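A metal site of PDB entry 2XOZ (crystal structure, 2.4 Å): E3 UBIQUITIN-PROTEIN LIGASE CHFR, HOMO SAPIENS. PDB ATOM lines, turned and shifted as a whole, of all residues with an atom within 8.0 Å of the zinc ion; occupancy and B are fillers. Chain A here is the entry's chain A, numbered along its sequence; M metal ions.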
ATOM      1  N   VAL A  23      12.604  -7.752 -18.518  1.00  0.00           N
ATOM      2  CA  VAL A  23      13.016  -9.001 -17.898  1.00  0.00           C
ATOM      3  C   VAL A  23      11.960  -9.396 -16.905  1.00  0.00           C
ATOM      4  O   VAL A  23      11.532  -8.586 -16.108  1.00  0.00           O
ATOM      5  CB  VAL A  23      14.371  -8.857 -17.178  1.00  0.00           C
ATOM      6  CG1 VAL A  23      14.619 -10.027 -16.251  1.00  0.00           C
ATOM      7  CG2 VAL A  23      15.497  -8.736 -18.189  1.00  0.00           C
ATOM      8  N   VAL A  24      11.514 -10.639 -16.954  1.00  0.00           N
ATOM      9  CA  VAL A  24      10.616 -11.178 -15.940  1.00  0.00           C
ATOM     10  C   VAL A  24      11.214 -12.426 -15.290  1.00  0.00           C
ATOM     11  O   VAL A  24      11.541 -13.393 -15.977  1.00  0.00           O
ATOM     12  CB  VAL A  24       9.248 -11.531 -16.544  1.00  0.00           C
ATOM     13  CG1 VAL A  24       8.428 -12.337 -15.539  1.00  0.00           C
ATOM     14  CG2 VAL A  24       8.505 -10.262 -16.979  1.00  0.00           C
ATOM     15  N   CYS A  25      11.345 -12.405 -13.972  1.00  0.00           N
ATOM     16  CA  CYS A  25      11.907 -13.535 -13.240  1.00  0.00           C
ATOM     17  C   CYS A  25      10.899 -14.160 -12.280  1.00  0.00           C
ATOM     18  O   CYS A  25       9.857 -13.576 -11.992  1.00  0.00           O
ATOM     19  CB  CYS A  25      13.159 -13.117 -12.462  1.00  0.00           C
ATOM     20  SG  CYS A  25      12.840 -12.439 -10.818  1.00  0.00           S
ATOM     21  N   ARG A  26      11.224 -15.358 -11.780  1.00  0.00           N
ATOM     22  CA  ARG A  26      10.400 -16.044 -10.769  1.00  0.00           C
ATOM     23  C   ARG A  26       9.765 -15.110  -9.730  1.00  0.00           C
ATOM     24  O   ARG A  26       8.685 -15.401  -9.214  1.00  0.00           O
ATOM     25  CB  ARG A  26      11.247 -17.080 -10.016  1.00  0.00           C
ATOM     26  CG  ARG A  26      11.546 -18.373 -10.745  1.00  0.00           C
ATOM     27  CD  ARG A  26      12.108 -19.407  -9.779  1.00  0.00           C
ATOM     28  NE  ARG A  26      13.272 -20.072 -10.357  1.00  0.00           N
ATOM     29  CZ  ARG A  26      14.019 -20.974  -9.712  1.00  0.00           C
ATOM     30  NH1 ARG A  26      13.722 -21.304  -8.466  1.00  0.00           N
ATOM     31  NH2 ARG A  26      15.070 -21.538 -10.326  1.00  0.00           N
ATOM     32  N   GLN A  27      10.432 -13.997  -9.395  1.00  0.00           N
ATOM     33  CA  GLN A  27      10.006 -13.139  -8.282  1.00  0.00           C
ATOM     34  C   GLN A  27       9.532 -11.758  -8.718  1.00  0.00           C
ATOM     35  O   GLN A  27       9.310 -10.873  -7.892  1.00  0.00           O
ATOM     36  CB  GLN A  27      11.128 -13.003  -7.244  1.00  0.00           C
ATOM     37  CG  GLN A  27      11.406 -14.266  -6.457  1.00  0.00           C
ATOM     38  CD  GLN A  27      12.578 -14.117  -5.486  1.00  0.00           C
ATOM     39  OE1 GLN A  27      13.379 -13.185  -5.604  1.00  0.00           O
ATOM     40  NE2 GLN A  27      12.681 -15.044  -4.537  1.00  0.00           N
ATOM     41  N   CYS A  28       9.403 -11.574 -10.028  1.00  0.00           N
ATOM     42  CA  CYS A  28       8.828 -10.342 -10.552  1.00  0.00           C
ATOM     43  C   CYS A  28       7.316 -10.321 -10.270  1.00  0.00           C
ATOM     44  O   CYS A  28       6.657 -11.373 -10.248  1.00  0.00           O
ATOM     45  CB  CYS A  28       9.109 -10.230 -12.052  1.00  0.00           C
ATOM     46  SG  CYS A  28      10.546  -9.207 -12.543  1.00  0.00           S
ATOM     47  N   PRO A  29       6.779  -9.114 -10.014  1.00  0.00           N
ATOM     48  CA  PRO A  29       5.353  -8.854  -9.749  1.00  0.00           C
ATOM     49  C   PRO A  29       4.440  -9.162 -10.947  1.00  0.00           C
ATOM     50  O   PRO A  29       4.854  -8.952 -12.089  1.00  0.00           O
ATOM     51  CB  PRO A  29       5.323  -7.355  -9.444  1.00  0.00           C
ATOM     52  CG  PRO A  29       6.549  -6.811 -10.133  1.00  0.00           C
ATOM     53  CD  PRO A  29       7.581  -7.878  -9.970  1.00  0.00           C
ATOM     54  N   ARG A  32       4.114  -6.979 -14.091  1.00  0.00           N
ATOM     55  CA  ARG A  32       5.249  -7.000 -15.004  1.00  0.00           C
ATOM     56  C   ARG A  32       5.103  -8.150 -16.006  1.00  0.00           C
ATOM     57  O   ARG A  32       5.367  -7.994 -17.190  1.00  0.00           O
ATOM     58  CB  ARG A  32       6.554  -7.150 -14.232  1.00  0.00           C
ATOM     59  CG  ARG A  32       7.047  -5.887 -13.560  1.00  0.00           C
ATOM     60  CD  ARG A  32       8.057  -5.165 -14.433  1.00  0.00           C
ATOM     61  NE  ARG A  32       9.326  -5.892 -14.565  1.00  0.00           N
ATOM     62  CZ  ARG A  32      10.342  -5.477 -15.313  1.00  0.00           C
ATOM     63  NH1 ARG A  32      10.247  -4.343 -16.003  1.00  0.00           N
ATOM     64  NH2 ARG A  32      11.470  -6.187 -15.385  1.00  0.00           N
ATOM     65  N   TYR A  71      10.319 -12.642  -1.392  1.00  0.00           N
ATOM     66  CA  TYR A  71      10.757 -11.407  -2.068  1.00  0.00           C
ATOM     67  C   TYR A  71       9.981 -11.114  -3.360  1.00  0.00           C
ATOM     68  O   TYR A  71       9.562 -12.025  -4.075  1.00  0.00           O
ATOM     69  CB  TYR A  71      12.266 -11.489  -2.354  1.00  0.00           C
ATOM     70  CG  TYR A  71      12.920 -10.247  -2.940  1.00  0.00           C
ATOM     71  CD1 TYR A  71      13.113 -10.124  -4.312  1.00  0.00           C
ATOM     72  CD2 TYR A  71      13.373  -9.210  -2.124  1.00  0.00           C
ATOM     73  CE1 TYR A  71      13.739  -9.005  -4.851  1.00  0.00           C
ATOM     74  CE2 TYR A  71      13.998  -8.087  -2.654  1.00  0.00           C
ATOM     75  CZ  TYR A  71      14.178  -7.991  -4.026  1.00  0.00           C
ATOM     76  OH  TYR A  71      14.805  -6.872  -4.565  1.00  0.00           O
ATOM     77  N   VAL A  72       9.790  -9.817  -3.649  1.00  0.00           N
ATOM     78  CA  VAL A  72       9.162  -9.357  -4.888  1.00  0.00           C
ATOM     79  C   VAL A  72      10.020  -8.246  -5.452  1.00  0.00           C
ATOM     80  O   VAL A  72      10.257  -7.245  -4.780  1.00  0.00           O
ATOM     81  CB  VAL A  72       7.761  -8.759  -4.644  1.00  0.00           C
ATOM     82  CG1 VAL A  72       7.264  -8.070  -5.900  1.00  0.00           C
ATOM     83  CG2 VAL A  72       6.777  -9.827  -4.191  1.00  0.00           C
ATOM     84  N   CYS A  73      10.491  -8.400  -6.681  1.00  0.00           N
ATOM     85  CA  CYS A  73      11.313  -7.371  -7.312  1.00  0.00           C
ATOM     86  C   CYS A  73      10.646  -5.996  -7.323  1.00  0.00           C
ATOM     87  O   CYS A  73       9.496  -5.860  -7.755  1.00  0.00           O
ATOM     88  CB  CYS A  73      11.667  -7.758  -8.748  1.00  0.00           C
ATOM     89  SG  CYS A  73      12.381  -9.391  -8.926  1.00  0.00           S
ATOM     90  N   PRO A  74      11.377  -4.964  -6.868  1.00  0.00           N
ATOM     91  CA  PRO A  74      10.964  -3.562  -6.919  1.00  0.00           C
ATOM     92  C   PRO A  74      11.231  -2.949  -8.280  1.00  0.00           C
ATOM     93  O   PRO A  74      11.888  -3.577  -9.121  1.00  0.00           O
ATOM     94  CB  PRO A  74      11.868  -2.897  -5.882  1.00  0.00           C
ATOM     95  CG  PRO A  74      13.115  -3.693  -5.936  1.00  0.00           C
ATOM     96  CD  PRO A  74      12.696  -5.118  -6.239  1.00  0.00           C
ATOM     97  N   GLY A  77      15.039  -1.938  -8.802  1.00  0.00           N
ATOM     98  CA  GLY A  77      15.962  -3.057  -8.698  1.00  0.00           C
ATOM     99  C   GLY A  77      16.400  -3.625 -10.038  1.00  0.00           C
ATOM    100  O   GLY A  77      15.752  -3.393 -11.061  1.00  0.00           O
ATOM    101  N   SER A  78      17.505  -4.367 -10.029  1.00  0.00           N
ATOM    102  CA  SER A  78      18.046  -4.935 -11.272  1.00  0.00           C
ATOM    103  C   SER A  78      18.060  -6.469 -11.232  1.00  0.00           C
ATOM    104  O   SER A  78      17.917  -7.063 -10.177  1.00  0.00           O
ATOM    105  CB  SER A  78      19.455  -4.394 -11.554  1.00  0.00           C
ATOM    106  OG  SER A  78      20.409  -4.850 -10.603  1.00  0.00           O
ATOM    107  N   HIS A  79      18.219  -7.090 -12.398  1.00  0.00           N
ATOM    108  CA  HIS A  79      18.355  -8.536 -12.473  1.00  0.00           C
ATOM    109  C   HIS A  79      19.755  -8.942 -12.963  1.00  0.00           C
ATOM    110  O   HIS A  79      20.417  -8.182 -13.675  1.00  0.00           O
ATOM    111  CB  HIS A  79      17.277  -9.145 -13.385  1.00  0.00           C
ATOM    112  CG  HIS A  79      15.867  -8.878 -12.928  1.00  0.00           C
ATOM    113  ND1 HIS A  79      15.240  -7.665 -13.122  1.00  0.00           N
ATOM    114  CD2 HIS A  79      14.966  -9.673 -12.305  1.00  0.00           C
ATOM    115  CE1 HIS A  79      14.012  -7.731 -12.633  1.00  0.00           C
ATOM    116  NE2 HIS A  79      13.828  -8.935 -12.136  1.00  0.00           N
ATOM    117  N   ALA A  80      20.212 -10.123 -12.563  1.00  0.00           N
ATOM    118  CA  ALA A  80      21.396 -10.713 -13.165  1.00  0.00           C
ATOM    119  C   ALA A  80      21.050 -12.088 -13.732  1.00  0.00           C
ATOM    120  O   ALA A  80      20.104 -12.725 -13.267  1.00  0.00           O
ATOM    121  CB  ALA A  80      22.536 -10.810 -12.152  1.00  0.00           C
ATOM    122  N   PRO A  88      17.134 -15.200 -15.377  1.00  0.00           N
ATOM    123  CA  PRO A  88      17.312 -13.974 -14.591  1.00  0.00           C
ATOM    124  C   PRO A  88      16.895 -14.152 -13.137  1.00  0.00           C
ATOM    125  O   PRO A  88      15.955 -14.871 -12.822  1.00  0.00           O
ATOM    126  CB  PRO A  88      16.376 -12.994 -15.274  1.00  0.00           C
ATOM    127  CG  PRO A  88      15.279 -13.877 -15.821  1.00  0.00           C
ATOM    128  CD  PRO A  88      16.018 -15.080 -16.341  1.00  0.00           C
ATOM    129  N   MET A  89      17.637 -13.498 -12.247  1.00  0.00           N
ATOM    130  CA  MET A  89      17.294 -13.431 -10.838  1.00  0.00           C
ATOM    131  C   MET A  89      17.478 -11.992 -10.433  1.00  0.00           C
ATOM    132  O   MET A  89      18.172 -11.236 -11.104  1.00  0.00           O
ATOM    133  CB  MET A  89      18.190 -14.353 -10.010  1.00  0.00           C
ATOM    134  CG  MET A  89      19.665 -14.010 -10.111  1.00  0.00           C
ATOM    135  SD  MET A  89      20.708 -15.185  -9.242  1.00  0.00           S
ATOM    136  CE  MET A  89      22.315 -14.669  -9.796  1.00  0.00           C
ATOM    137  N   PRO A  90      16.836 -11.604  -9.330  1.00  0.00           N
ATOM    138  CA  PRO A  90      16.980 -10.243  -8.812  1.00  0.00           C
ATOM    139  C   PRO A  90      18.394 -10.114  -8.336  1.00  0.00           C
ATOM    140  O   PRO A  90      18.887 -11.038  -7.687  1.00  0.00           O
ATOM    141  CB  PRO A  90      16.028 -10.223  -7.617  1.00  0.00           C
ATOM    142  CG  PRO A  90      15.951 -11.645  -7.183  1.00  0.00           C
ATOM    143  CD  PRO A  90      15.973 -12.431  -8.469  1.00  0.00           C
ATOM    144  N   ASP A  91      19.065  -9.013  -8.676  1.00  0.00           N
ATOM    145  CA  ASP A  91      20.441  -8.822  -8.261  1.00  0.00           C
ATOM    146  C   ASP A  91      20.508  -8.201  -6.875  1.00  0.00           C
ATOM    147  O   ASP A  91      20.357  -6.991  -6.727  1.00  0.00           O
ATOM    148  CB  ASP A  91      21.228  -7.975  -9.259  1.00  0.00           C
ATOM    149  CG  ASP A  91      22.714  -8.008  -8.982  1.00  0.00           C
ATOM    150  OD1 ASP A  91      23.520  -7.863  -9.934  1.00  0.00           O
ATOM    151  OD2 ASP A  91      23.084  -8.224  -7.809  1.00  0.00           O
ATOM    152  N   TRP A 119      17.705 -19.578  -4.859  1.00  0.00           N
ATOM    153  CA  TRP A 119      16.383 -20.178  -5.021  1.00  0.00           C
ATOM    154  C   TRP A 119      16.345 -21.533  -5.729  1.00  0.00           C
ATOM    155  O   TRP A 119      15.287 -21.988  -6.126  1.00  0.00           O
ATOM    156  CB  TRP A 119      15.416 -19.198  -5.708  1.00  0.00           C
ATOM    157  CG  TRP A 119      15.773 -18.818  -7.129  1.00  0.00           C
ATOM    158  CD1 TRP A 119      16.609 -19.486  -7.965  1.00  0.00           C
ATOM    159  CD2 TRP A 119      15.255 -17.694  -7.873  1.00  0.00           C
ATOM    160  NE1 TRP A 119      16.666 -18.842  -9.184  1.00  0.00           N
ATOM    161  CE2 TRP A 119      15.841 -17.745  -9.147  1.00  0.00           C
ATOM    162  CE3 TRP A 119      14.362 -16.665  -7.584  1.00  0.00           C
ATOM    163  CZ2 TRP A 119      15.565 -16.795 -10.136  1.00  0.00           C
ATOM    164  CZ3 TRP A 119      14.087 -15.719  -8.560  1.00  0.00           C
ATOM    165  CH2 TRP A 119      14.687 -15.779  -9.815  1.00  0.00           C
HETATM  166 ZN    ZN M   1      12.447 -10.136 -11.169  1.00  0.00          ZN
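Within 4 Å of the zinc ion: Cys 25, Cys 28, Cys 73 and His 79.
The backbone NH (N) of Gln 27 lies close to the side-chain sulfur (SG) of Cys 25 (3.2 Å). O of Gln 27 sits at hydrogen-bond distance from N of Cys 73. The backbone carbonyl oxygen (O) of Val 23 sits close to the side-chain sulfur (SG) of Cys 28 (3.8 Å).
The zinc ion is bound by a ring nitrogen (NE2) of His 79 (2.1 Å), the side-chain sulfur (SG) of Cys 25 (2.4 Å), the side-chain sulfur (SG) of Cys 73 (2.4 Å) and the side-chain sulfur (SG) of Cys 28 (2.5 Å).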
